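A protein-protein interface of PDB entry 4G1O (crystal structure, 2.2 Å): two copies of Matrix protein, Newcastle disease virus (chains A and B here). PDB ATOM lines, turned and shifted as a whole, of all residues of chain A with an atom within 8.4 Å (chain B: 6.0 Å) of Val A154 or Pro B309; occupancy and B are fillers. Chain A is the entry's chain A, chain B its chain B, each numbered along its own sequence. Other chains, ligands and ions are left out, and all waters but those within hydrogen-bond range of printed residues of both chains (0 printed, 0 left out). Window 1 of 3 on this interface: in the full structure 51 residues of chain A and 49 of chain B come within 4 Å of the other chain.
Of chain B, only Pro B309 (3.8 Å) and Gln B310 (3.6 Å) come within 4 Å of Val A154. Of chain A, only Val A154 comes within 4 Å of Pro B309. Of chain A, only Glu A125 comes within 4 Å of Ser B308. Printed residues of chain B within 4 Å of Lys A158: Gln B310 (3.1 Å). Of the printed residues of chain B, Thr A124 touches Asn B306 and Ala B307. Of the printed residues of chain B, Glu A125 touches Ala B307 (3.0 Å) and Ser B308 (3.5 Å). Printed residues of chain B within 4 Å of Glu A161: Gln B310, Val B311 and Ile B314. The nearest residue of chain B that does not touch Val A154 is Ser B308 (5.7 Å). The nearest printed residue of chain B that does not touch Glu A125 is Asn B306 (5.0 Å).
The backbone carbonyl oxygen of Lys A158 lies within hydrogen-bond range of the side-chain amino group of Lys A313. O of Glu A125 lies within hydrogen-bond range of N of Ala A153, 3.0 Å away. OD1 of Asn A152 is in hydrogen-bond range of N of Val A154 (3.0 Å). The side-chain amino group (NZ) of Lys A313 lies within hydrogen-bond range of the backbone carbonyl oxygen (O) of Val A157 (2.9 Å). The side-chain amino group of Lys A313 sits close to the backbone carbonyl oxygen of Val A154 (3.0 Å). The side-chain amino group (NZ) of Lys B313 sits at hydrogen-bond distance from the backbone carbonyl oxygen (O) of Val B154 (2.7 Å).
O of Lys A158 lies close to OE1 of Gln B310 (3.1 Å). The side-chain amino group of Lys A313 lies close to the side-chain amide nitrogen of Gln B310, at 3.0 Å. NZ of Lys B313 lies close to NE2 of Gln A310, at 3.0 Å. O of Ala B307 lies within hydrogen-bond range of N of Glu A125 (3.0 Å). The side-chain carboxylate (OE1) of Glu A125 sits at hydrogen-bond distance from the side-chain hydroxyl (OG) of Ser B308 (3.5 Å). OE1 of Gln B310 lies close to OE1 of Glu A161, 3.5 Å away.
O of Asn B306 touches CB of Thr A124 (3.4 Å). O of Ala B307 touches CA of Thr A124 (3.9 Å). CG1 of Val A154 touches CG of Pro B309 (3.8 Å). Val A154 touches Gln B310 (CG2 to NE2, 3.6 Å). Glu A161 touches Val B311. Glu A161 touches Ile B314 (OE2 to CD1, 3.8 Å). CG2 of Val B154 touches CG of Gln A310 (3.8 Å).
Printed residues of chain B that touch a printed residue of chain A: Val B154, Asn B306, Ala B307, Ser B308, Pro B309, Gln B310, Val B311, Lys B313 and Ile B314.
Val A154 touches Pro B309, but with the chains exchanged Pro A309 does not touch Val B154 (4.1 Å). Val A154 touches Gln B310, and with the chains exchanged Gln A310 touches Val B154. Gln A310 touches Lys B313, and with the chains exchanged Lys A313 touches Gln B310. Positions printed for both chains: 154, 155, 305, 308, 309, 310, 312 and 313.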
ATOM      1  N   ALA A  89       0.545 -12.735 -25.015  1.00  0.00           N
ATOM      2  CA  ALA A  89      -0.364 -11.899 -24.201  1.00  0.00           C
ATOM      3  C   ALA A  89       0.422 -10.953 -23.294  1.00  0.00           C
ATOM      4  O   ALA A  89       1.625 -11.151 -23.068  1.00  0.00           O
ATOM      5  CB  ALA A  89      -1.280 -12.758 -23.348  1.00  0.00           C
ATOM      6  N   MET A  91      -0.254  -7.688 -19.922  1.00  0.00           N
ATOM      7  CA  MET A  91      -1.191  -6.953 -19.080  1.00  0.00           C
ATOM      8  C   MET A  91      -0.710  -5.533 -18.872  1.00  0.00           C
ATOM      9  O   MET A  91       0.494  -5.294 -18.787  1.00  0.00           O
ATOM     10  CB  MET A  91      -1.356  -7.629 -17.724  1.00  0.00           C
ATOM     11  CG  MET A  91      -0.381  -7.130 -16.669  1.00  0.00           C
ATOM     12  SD  MET A  91      -1.231  -6.570 -15.178  1.00  0.00           S
ATOM     13  CE  MET A  91      -1.810  -8.168 -14.667  1.00  0.00           C
ATOM     14  N   LYS A 119      10.706  -3.038 -26.456  1.00  0.00           N
ATOM     15  CA  LYS A 119      11.545  -3.502 -25.352  1.00  0.00           C
ATOM     16  C   LYS A 119      12.471  -2.371 -24.973  1.00  0.00           C
ATOM     17  O   LYS A 119      12.839  -1.552 -25.799  1.00  0.00           O
ATOM     18  CB  LYS A 119      12.433  -4.699 -25.752  1.00  0.00           C
ATOM     19  CG  LYS A 119      11.707  -5.978 -26.100  1.00  0.00           C
ATOM     20  CD  LYS A 119      11.658  -6.962 -24.958  1.00  0.00           C
ATOM     21  CE  LYS A 119      12.658  -8.072 -25.216  1.00  0.00           C
ATOM     22  NZ  LYS A 119      12.091  -9.387 -24.809  1.00  0.00           N
ATOM     23  N   THR A 124      16.679  -4.775 -15.524  1.00  0.00           N
ATOM     24  CA  THR A 124      16.046  -5.978 -16.139  1.00  0.00           C
ATOM     25  C   THR A 124      15.414  -5.521 -17.438  1.00  0.00           C
ATOM     26  O   THR A 124      15.305  -4.303 -17.636  1.00  0.00           O
ATOM     27  CB  THR A 124      14.961  -6.581 -15.244  1.00  0.00           C
ATOM     28  N   GLU A 125      14.984  -6.475 -18.287  1.00  0.00           N
ATOM     29  CA  GLU A 125      14.148  -6.180 -19.459  1.00  0.00           C
ATOM     30  C   GLU A 125      12.893  -5.407 -19.070  1.00  0.00           C
ATOM     31  O   GLU A 125      12.192  -5.796 -18.125  1.00  0.00           O
ATOM     32  CB  GLU A 125      13.675  -7.455 -20.147  1.00  0.00           C
ATOM     33  CG  GLU A 125      14.564  -7.966 -21.262  1.00  0.00           C
ATOM     34  CD  GLU A 125      13.919  -9.098 -22.079  1.00  0.00           C
ATOM     35  OE1 GLU A 125      13.043  -9.817 -21.540  1.00  0.00           O
ATOM     36  OE2 GLU A 125      14.293  -9.269 -23.264  1.00  0.00           O
ATOM     37  N   ARG A 126      12.596  -4.344 -19.828  1.00  0.00           N
ATOM     38  CA  ARG A 126      11.356  -3.573 -19.661  1.00  0.00           C
ATOM     39  C   ARG A 126      10.477  -3.638 -20.909  1.00  0.00           C
ATOM     40  O   ARG A 126      10.992  -3.774 -22.035  1.00  0.00           O
ATOM     41  CB  ARG A 126      11.661  -2.111 -19.367  1.00  0.00           C
ATOM     42  CG  ARG A 126      12.961  -1.927 -18.621  1.00  0.00           C
ATOM     43  CD  ARG A 126      12.747  -0.989 -17.477  1.00  0.00           C
ATOM     44  NE  ARG A 126      11.642  -1.452 -16.670  1.00  0.00           N
ATOM     45  CZ  ARG A 126      11.167  -0.747 -15.664  1.00  0.00           C
ATOM     46  NH1 ARG A 126      11.743   0.428 -15.392  1.00  0.00           N
ATOM     47  NH2 ARG A 126      10.143  -1.206 -14.940  1.00  0.00           N
ATOM     48  N   MET A 127       9.158  -3.559 -20.707  1.00  0.00           N
ATOM     49  CA  MET A 127       8.249  -3.356 -21.806  1.00  0.00           C
ATOM     50  C   MET A 127       7.734  -1.930 -21.652  1.00  0.00           C
ATOM     51  O   MET A 127       7.241  -1.513 -20.571  1.00  0.00           O
ATOM     52  CB  MET A 127       7.135  -4.422 -21.798  1.00  0.00           C
ATOM     53  CG  MET A 127       6.413  -4.672 -23.122  1.00  0.00           C
ATOM     54  SD  MET A 127       7.387  -5.118 -24.588  1.00  0.00           S
ATOM     55  CE  MET A 127       8.590  -6.191 -23.849  1.00  0.00           C
ATOM     56  N   VAL A 151       7.445  -0.901 -17.794  1.00  0.00           N
ATOM     57  CA  VAL A 151       7.222  -1.898 -16.767  1.00  0.00           C
ATOM     58  C   VAL A 151       8.131  -3.090 -16.924  1.00  0.00           C
ATOM     59  O   VAL A 151       8.648  -3.376 -18.020  1.00  0.00           O
ATOM     60  CB  VAL A 151       5.749  -2.386 -16.701  1.00  0.00           C
ATOM     61  CG1 VAL A 151       4.819  -1.320 -16.128  1.00  0.00           C
ATOM     62  CG2 VAL A 151       5.262  -2.845 -18.054  1.00  0.00           C
ATOM     63  N   ASN A 152       8.288  -3.797 -15.809  1.00  0.00           N
ATOM     64  CA  ASN A 152       9.105  -4.969 -15.757  1.00  0.00           C
ATOM     65  C   ASN A 152       8.472  -5.960 -16.692  1.00  0.00           C
ATOM     66  O   ASN A 152       7.319  -6.323 -16.511  1.00  0.00           O
ATOM     67  CB  ASN A 152       9.140  -5.548 -14.343  1.00  0.00           C
ATOM     68  CG  ASN A 152       9.816  -6.918 -14.306  1.00  0.00           C
ATOM     69  OD1 ASN A 152       9.402  -7.869 -14.985  1.00  0.00           O
ATOM     70  ND2 ASN A 152      10.861  -7.014 -13.544  1.00  0.00           N
ATOM     71  N   ALA A 153       9.245  -6.385 -17.674  1.00  0.00           N
ATOM     72  CA  ALA A 153       8.765  -7.150 -18.809  1.00  0.00           C
ATOM     73  C   ALA A 153       8.228  -8.512 -18.411  1.00  0.00           C
ATOM     74  O   ALA A 153       7.132  -8.889 -18.830  1.00  0.00           O
ATOM     75  CB  ALA A 153       9.880  -7.306 -19.861  1.00  0.00           C
ATOM     76  N   VAL A 154       8.999  -9.270 -17.629  1.00  0.00           N
ATOM     77  CA  VAL A 154       8.593 -10.645 -17.336  1.00  0.00           C
ATOM     78  C   VAL A 154       7.276 -10.669 -16.547  1.00  0.00           C
ATOM     79  O   VAL A 154       6.498 -11.616 -16.655  1.00  0.00           O
ATOM     80  CB  VAL A 154       9.724 -11.513 -16.718  1.00  0.00           C
ATOM     81  CG1 VAL A 154      10.074 -11.054 -15.313  1.00  0.00           C
ATOM     82  CG2 VAL A 154       9.363 -13.005 -16.763  1.00  0.00           C
ATOM     83  N   LYS A 155       7.024  -9.600 -15.796  1.00  0.00           N
ATOM     84  CA  LYS A 155       5.756  -9.423 -15.072  1.00  0.00           C
ATOM     85  C   LYS A 155       4.562  -8.985 -15.929  1.00  0.00           C
ATOM     86  O   LYS A 155       3.418  -9.144 -15.509  1.00  0.00           O
ATOM     87  CB  LYS A 155       5.927  -8.407 -13.932  1.00  0.00           C
ATOM     88  CG  LYS A 155       6.682  -8.921 -12.721  1.00  0.00           C
ATOM     89  CD  LYS A 155       7.174  -7.763 -11.869  1.00  0.00           C
ATOM     90  CE  LYS A 155       8.229  -8.268 -10.895  1.00  0.00           C
ATOM     91  NZ  LYS A 155       8.193  -7.445  -9.665  1.00  0.00           N
ATOM     92  N   HIS A 156       4.808  -8.405 -17.097  1.00  0.00           N
ATOM     93  CA  HIS A 156       3.704  -7.870 -17.909  1.00  0.00           C
ATOM     94  C   HIS A 156       3.525  -8.499 -19.269  1.00  0.00           C
ATOM     95  O   HIS A 156       2.605  -8.147 -19.987  1.00  0.00           O
ATOM     96  CB  HIS A 156       3.804  -6.351 -18.015  1.00  0.00           C
ATOM     97  CG  HIS A 156       3.751  -5.665 -16.665  1.00  0.00           C
ATOM     98  ND1 HIS A 156       2.611  -5.150 -16.156  1.00  0.00           N
ATOM     99  CD2 HIS A 156       4.741  -5.473 -15.696  1.00  0.00           C
ATOM    100  CE1 HIS A 156       2.863  -4.644 -14.936  1.00  0.00           C
ATOM    101  NE2 HIS A 156       4.172  -4.843 -14.665  1.00  0.00           N
ATOM    102  N   VAL A 157       4.408  -9.426 -19.630  1.00  0.00           N
ATOM    103  CA  VAL A 157       4.360 -10.088 -20.935  1.00  0.00           C
ATOM    104  C   VAL A 157       4.527 -11.570 -20.659  1.00  0.00           C
ATOM    105  O   VAL A 157       5.389 -11.942 -19.870  1.00  0.00           O
ATOM    106  CB  VAL A 157       5.486  -9.609 -21.884  1.00  0.00           C
ATOM    107  CG1 VAL A 157       5.504 -10.443 -23.153  1.00  0.00           C
ATOM    108  CG2 VAL A 157       5.326  -8.126 -22.221  1.00  0.00           C
ATOM    109  N   LYS A 158       3.717 -12.417 -21.295  1.00  0.00           N
ATOM    110  CA  LYS A 158       3.761 -13.846 -21.013  1.00  0.00           C
ATOM    111  C   LYS A 158       5.058 -14.526 -21.464  1.00  0.00           C
ATOM    112  O   LYS A 158       5.706 -15.246 -20.682  1.00  0.00           O
ATOM    113  CB  LYS A 158       2.545 -14.548 -21.609  1.00  0.00           C
ATOM    114  CG  LYS A 158       2.416 -15.986 -21.128  1.00  0.00           C
ATOM    115  CD  LYS A 158       1.621 -16.165 -19.830  1.00  0.00           C
ATOM    116  CE  LYS A 158       1.608 -17.659 -19.447  1.00  0.00           C
ATOM    117  NZ  LYS A 158       0.839 -18.135 -18.248  1.00  0.00           N
ATOM    118  N   ALA A 159       5.430 -14.299 -22.725  1.00  0.00           N
ATOM    119  CA  ALA A 159       6.707 -14.776 -23.246  1.00  0.00           C
ATOM    120  C   ALA A 159       7.591 -13.619 -23.773  1.00  0.00           C
ATOM    121  O   ALA A 159       7.734 -13.444 -24.993  1.00  0.00           O
ATOM    122  CB  ALA A 159       6.480 -15.846 -24.314  1.00  0.00           C
ATOM    123  N   PRO A 160       8.203 -12.833 -22.858  1.00  0.00           N
ATOM    124  CA  PRO A 160       9.105 -11.794 -23.353  1.00  0.00           C
ATOM    125  C   PRO A 160      10.232 -12.346 -24.274  1.00  0.00           C
ATOM    126  O   PRO A 160      10.686 -11.639 -25.185  1.00  0.00           O
ATOM    127  CB  PRO A 160       9.672 -11.149 -22.074  1.00  0.00           C
ATOM    128  CG  PRO A 160       9.340 -12.068 -20.939  1.00  0.00           C
ATOM    129  CD  PRO A 160       8.185 -12.923 -21.382  1.00  0.00           C
ATOM    130  N   GLU A 161      10.653 -13.599 -24.069  1.00  0.00           N
ATOM    131  CA  GLU A 161      11.649 -14.248 -24.963  1.00  0.00           C
ATOM    132  C   GLU A 161      11.203 -14.343 -26.435  1.00  0.00           C
ATOM    133  O   GLU A 161      12.019 -14.635 -27.331  1.00  0.00           O
ATOM    134  CB  GLU A 161      12.075 -15.625 -24.429  1.00  0.00           C
ATOM    135  CG  GLU A 161      10.966 -16.679 -24.357  1.00  0.00           C
ATOM    136  CD  GLU A 161      10.155 -16.694 -23.053  1.00  0.00           C
ATOM    137  OE1 GLU A 161       9.922 -15.605 -22.463  1.00  0.00           O
ATOM    138  OE2 GLU A 161       9.726 -17.806 -22.633  1.00  0.00           O
ATOM    139  N   SER A 305       2.366 -10.272  -8.935  1.00  0.00           N
ATOM    140  CA  SER A 305       3.405  -9.988  -9.905  1.00  0.00           C
ATOM    141  C   SER A 305       4.774  -9.836  -9.200  1.00  0.00           C
ATOM    142  O   SER A 305       5.813 -10.298  -9.724  1.00  0.00           O
ATOM    143  CB  SER A 305       3.038  -8.687 -10.673  1.00  0.00           C
ATOM    144  N   SER A 308       4.984 -13.564  -6.722  1.00  0.00           N
ATOM    145  CA  SER A 308       5.313 -14.735  -7.530  1.00  0.00           C
ATOM    146  C   SER A 308       4.923 -14.514  -9.010  1.00  0.00           C
ATOM    147  O   SER A 308       3.823 -14.808  -9.407  1.00  0.00           O
ATOM    148  CB  SER A 308       4.598 -15.964  -6.911  1.00  0.00           C
ATOM    149  OG  SER A 308       4.578 -17.116  -7.743  1.00  0.00           O
ATOM    150  N   PRO A 309       5.834 -13.989  -9.841  1.00  0.00           N
ATOM    151  CA  PRO A 309       5.432 -13.644 -11.204  1.00  0.00           C
ATOM    152  C   PRO A 309       4.708 -14.766 -12.002  1.00  0.00           C
ATOM    153  O   PRO A 309       3.867 -14.450 -12.846  1.00  0.00           O
ATOM    154  CB  PRO A 309       6.741 -13.279 -11.880  1.00  0.00           C
ATOM    155  CG  PRO A 309       7.687 -12.921 -10.771  1.00  0.00           C
ATOM    156  CD  PRO A 309       7.223 -13.602  -9.532  1.00  0.00           C
ATOM    157  N   GLN A 310       5.013 -16.039 -11.752  1.00  0.00           N
ATOM    158  CA  GLN A 310       4.435 -17.122 -12.565  1.00  0.00           C
ATOM    159  C   GLN A 310       2.982 -17.402 -12.204  1.00  0.00           C
ATOM    160  O   GLN A 310       2.204 -17.876 -13.029  1.00  0.00           O
ATOM    161  CB  GLN A 310       5.278 -18.412 -12.504  1.00  0.00           C
ATOM    162  CG  GLN A 310       6.699 -18.226 -13.007  1.00  0.00           C
ATOM    163  CD  GLN A 310       7.281 -19.426 -13.729  1.00  0.00           C
ATOM    164  OE1 GLN A 310       6.690 -20.529 -13.763  1.00  0.00           O
ATOM    165  NE2 GLN A 310       8.451 -19.214 -14.339  1.00  0.00           N
ATOM    166  N   ALA A 312       0.993 -14.919 -10.875  1.00  0.00           N
ATOM    167  CA  ALA A 312       0.246 -13.786 -11.340  1.00  0.00           C
ATOM    168  C   ALA A 312      -0.140 -14.017 -12.792  1.00  0.00           C
ATOM    169  O   ALA A 312      -1.282 -13.797 -13.154  1.00  0.00           O
ATOM    170  CB  ALA A 312       1.052 -12.509 -11.176  1.00  0.00           C
ATOM    171  N   LYS A 313       0.786 -14.514 -13.609  1.00  0.00           N
ATOM    172  CA  LYS A 313       0.494 -14.741 -15.043  1.00  0.00           C
ATOM    173  C   LYS A 313      -0.536 -15.853 -15.332  1.00  0.00           C
ATOM    174  O   LYS A 313      -1.321 -15.761 -16.296  1.00  0.00           O
ATOM    175  CB  LYS A 313       1.797 -14.898 -15.846  1.00  0.00           C
ATOM    176  CG  LYS A 313       2.712 -13.658 -15.740  1.00  0.00           C
ATOM    177  CD  LYS A 313       3.608 -13.443 -16.953  1.00  0.00           C
ATOM    178  CE  LYS A 313       4.941 -14.143 -16.774  1.00  0.00           C
ATOM    179  NZ  LYS A 313       5.707 -14.117 -18.049  1.00  0.00           N
ATOM    180  N   TRP A 316      -3.910 -14.406 -15.084  1.00  0.00           N
ATOM    181  CA  TRP A 316      -4.403 -13.626 -16.243  1.00  0.00           C
ATOM    182  C   TRP A 316      -5.574 -14.270 -16.971  1.00  0.00           C
ATOM    183  O   TRP A 316      -6.523 -13.580 -17.400  1.00  0.00           O
ATOM    184  CB  TRP A 316      -3.303 -13.452 -17.267  1.00  0.00           C
ATOM    185  CG  TRP A 316      -2.196 -12.524 -16.869  1.00  0.00           C
ATOM    186  CD1 TRP A 316      -1.997 -11.891 -15.642  1.00  0.00           C
ATOM    187  CD2 TRP A 316      -1.051 -12.126 -17.701  1.00  0.00           C
ATOM    188  NE1 TRP A 316      -0.842 -11.130 -15.675  1.00  0.00           N
ATOM    189  CE2 TRP A 316      -0.227 -11.234 -16.866  1.00  0.00           C
ATOM    190  CE3 TRP A 316      -0.644 -12.401 -19.014  1.00  0.00           C
ATOM    191  CZ2 TRP A 316       0.941 -10.660 -17.334  1.00  0.00           C
ATOM    192  CZ3 TRP A 316       0.537 -11.805 -19.476  1.00  0.00           C
ATOM    193  CH2 TRP A 316       1.298 -10.952 -18.658  1.00  0.00           C
ATOM    194  N   VAL B 154      11.665 -17.397  -8.244  1.00  0.00           N
ATOM    195  CA  VAL B 154      11.340 -17.490  -9.661  1.00  0.00           C
ATOM    196  C   VAL B 154      12.604 -17.681 -10.534  1.00  0.00           C
ATOM    197  O   VAL B 154      12.575 -18.415 -11.548  1.00  0.00           O
ATOM    198  CB  VAL B 154      10.408 -16.349 -10.128  1.00  0.00           C
ATOM    199  CG1 VAL B 154      11.114 -14.997 -10.101  1.00  0.00           C
ATOM    200  CG2 VAL B 154       9.876 -16.652 -11.514  1.00  0.00           C
ATOM    201  N   LYS B 155      13.720 -17.091 -10.113  1.00  0.00           N
ATOM    202  CA  LYS B 155      14.977 -17.187 -10.864  1.00  0.00           C
ATOM    203  C   LYS B 155      15.700 -18.526 -10.700  1.00  0.00           C
ATOM    204  O   LYS B 155      16.550 -18.883 -11.571  1.00  0.00           O
ATOM    205  CB  LYS B 155      15.936 -16.067 -10.432  1.00  0.00           C
ATOM    206  CG  LYS B 155      15.512 -14.694 -10.901  1.00  0.00           C
ATOM    207  CD  LYS B 155      16.250 -13.598 -10.169  1.00  0.00           C
ATOM    208  CE  LYS B 155      15.701 -12.256 -10.664  1.00  0.00           C
ATOM    209  NZ  LYS B 155      16.361 -11.184  -9.902  1.00  0.00           N
ATOM    210  N   ILE B 304      21.503 -13.781 -16.847  1.00  0.00           N
ATOM    211  CA  ILE B 304      20.253 -13.657 -17.560  1.00  0.00           C
ATOM    212  C   ILE B 304      19.106 -13.834 -16.580  1.00  0.00           C
ATOM    213  O   ILE B 304      18.023 -13.322 -16.800  1.00  0.00           O
ATOM    214  CB  ILE B 304      20.198 -14.642 -18.748  1.00  0.00           C
ATOM    215  CG1 ILE B 304      21.322 -14.309 -19.753  1.00  0.00           C
ATOM    216  CG2 ILE B 304      18.831 -14.574 -19.404  1.00  0.00           C
ATOM    217  CD1 ILE B 304      21.664 -15.419 -20.764  1.00  0.00           C
ATOM    218  N   SER B 305      19.356 -14.558 -15.497  1.00  0.00           N
ATOM    219  CA  SER B 305      18.410 -14.717 -14.369  1.00  0.00           C
ATOM    220  C   SER B 305      17.839 -13.350 -13.922  1.00  0.00           C
ATOM    221  O   SER B 305      16.650 -13.223 -13.614  1.00  0.00           O
ATOM    222  CB  SER B 305      19.088 -15.452 -13.190  1.00  0.00           C
ATOM    223  N   ASN B 306      18.669 -12.314 -13.917  1.00  0.00           N
ATOM    224  CA  ASN B 306      18.182 -10.985 -13.591  1.00  0.00           C
ATOM    225  C   ASN B 306      17.656 -10.240 -14.814  1.00  0.00           C
ATOM    226  O   ASN B 306      16.723  -9.475 -14.712  1.00  0.00           O
ATOM    227  CB  ASN B 306      19.284 -10.140 -12.949  1.00  0.00           C
ATOM    228  CG  ASN B 306      19.791 -10.724 -11.652  1.00  0.00           C
ATOM    229  OD1 ASN B 306      19.078 -11.462 -10.958  1.00  0.00           O
ATOM    230  ND2 ASN B 306      21.051 -10.402 -11.319  1.00  0.00           N
ATOM    231  N   ALA B 307      18.270 -10.434 -15.965  1.00  0.00           N
ATOM    232  CA  ALA B 307      17.820  -9.695 -17.154  1.00  0.00           C
ATOM    233  C   ALA B 307      16.491 -10.213 -17.689  1.00  0.00           C
ATOM    234  O   ALA B 307      15.554  -9.441 -17.945  1.00  0.00           O
ATOM    235  CB  ALA B 307      18.871  -9.735 -18.242  1.00  0.00           C
ATOM    236  N   SER B 308      16.410 -11.525 -17.860  1.00  0.00           N
ATOM    237  CA  SER B 308      15.190 -12.108 -18.361  1.00  0.00           C
ATOM    238  C   SER B 308      15.059 -13.518 -17.814  1.00  0.00           C
ATOM    239  O   SER B 308      15.604 -14.463 -18.406  1.00  0.00           O
ATOM    240  CB  SER B 308      15.198 -12.106 -19.882  1.00  0.00           C
ATOM    241  OG  SER B 308      14.129 -12.888 -20.360  1.00  0.00           O
ATOM    242  N   PRO B 309      14.345 -13.663 -16.675  1.00  0.00           N
ATOM    243  CA  PRO B 309      14.338 -14.930 -15.924  1.00  0.00           C
ATOM    244  C   PRO B 309      13.800 -16.103 -16.762  1.00  0.00           C
ATOM    245  O   PRO B 309      14.217 -17.250 -16.572  1.00  0.00           O
ATOM    246  CB  PRO B 309      13.426 -14.649 -14.696  1.00  0.00           C
ATOM    247  CG  PRO B 309      13.233 -13.150 -14.652  1.00  0.00           C
ATOM    248  CD  PRO B 309      13.703 -12.541 -15.955  1.00  0.00           C
ATOM    249  N   GLN B 310      12.864 -15.854 -17.648  1.00  0.00           N
ATOM    250  CA  GLN B 310      12.417 -16.907 -18.537  1.00  0.00           C
ATOM    251  C   GLN B 310      13.421 -17.388 -19.567  1.00  0.00           C
ATOM    252  O   GLN B 310      13.556 -18.561 -19.736  1.00  0.00           O
ATOM    253  CB  GLN B 310      11.028 -16.624 -19.081  1.00  0.00           C
ATOM    254  CG  GLN B 310      10.038 -16.643 -17.949  1.00  0.00           C
ATOM    255  CD  GLN B 310       8.632 -16.427 -18.370  1.00  0.00           C
ATOM    256  OE1 GLN B 310       8.317 -16.498 -19.525  1.00  0.00           O
ATOM    257  NE2 GLN B 310       7.774 -16.174 -17.425  1.00  0.00           N
ATOM    258  N   VAL B 311      14.158 -16.491 -20.204  1.00  0.00           N
ATOM    259  CA  VAL B 311      15.293 -16.884 -21.056  1.00  0.00           C
ATOM    260  C   VAL B 311      16.266 -17.731 -20.260  1.00  0.00           C
ATOM    261  O   VAL B 311      16.678 -18.798 -20.722  1.00  0.00           O
ATOM    262  CB  VAL B 311      16.038 -15.695 -21.719  1.00  0.00           C
ATOM    263  CG1 VAL B 311      17.377 -16.149 -22.325  1.00  0.00           C
ATOM    264  CG2 VAL B 311      15.175 -15.071 -22.811  1.00  0.00           C
ATOM    265  N   ALA B 312      16.630 -17.267 -19.071  1.00  0.00           N
ATOM    266  CA  ALA B 312      17.532 -18.030 -18.217  1.00  0.00           C
ATOM    267  C   ALA B 312      17.098 -19.466 -17.975  1.00  0.00           C
ATOM    268  O   ALA B 312      17.936 -20.352 -18.052  1.00  0.00           O
ATOM    269  CB  ALA B 312      17.762 -17.342 -16.872  1.00  0.00           C
ATOM    270  N   LYS B 313      15.834 -19.720 -17.643  1.00  0.00           N
ATOM    271  CA  LYS B 313      15.453 -21.118 -17.285  1.00  0.00           C
ATOM    272  C   LYS B 313      15.371 -22.022 -18.516  1.00  0.00           C
ATOM    273  O   LYS B 313      15.557 -23.255 -18.427  1.00  0.00           O
ATOM    274  CB  LYS B 313      14.194 -21.163 -16.416  1.00  0.00           C
ATOM    275  CG  LYS B 313      14.348 -20.205 -15.218  1.00  0.00           C
ATOM    276  CD  LYS B 313      13.377 -20.457 -14.082  1.00  0.00           C
ATOM    277  CE  LYS B 313      11.980 -19.959 -14.430  1.00  0.00           C
ATOM    278  NZ  LYS B 313      11.089 -19.951 -13.230  1.00  0.00           N
ATOM    279  N   ILE B 314      15.153 -21.411 -19.677  1.00  0.00           N
ATOM    280  CA  ILE B 314      15.186 -22.193 -20.934  1.00  0.00           C
ATOM    281  C   ILE B 314      16.606 -22.688 -21.083  1.00  0.00           C
ATOM    282  O   ILE B 314      16.819 -23.856 -21.370  1.00  0.00           O
ATOM    283  CB  ILE B 314      14.746 -21.408 -22.207  1.00  0.00           C
ATOM    284  CG1 ILE B 314      13.244 -21.073 -22.140  1.00  0.00           C
ATOM    285  CG2 ILE B 314      15.017 -22.219 -23.496  1.00  0.00           C
ATOM    286  CD1 ILE B 314      12.748 -20.080 -23.189  1.00  0.00           C
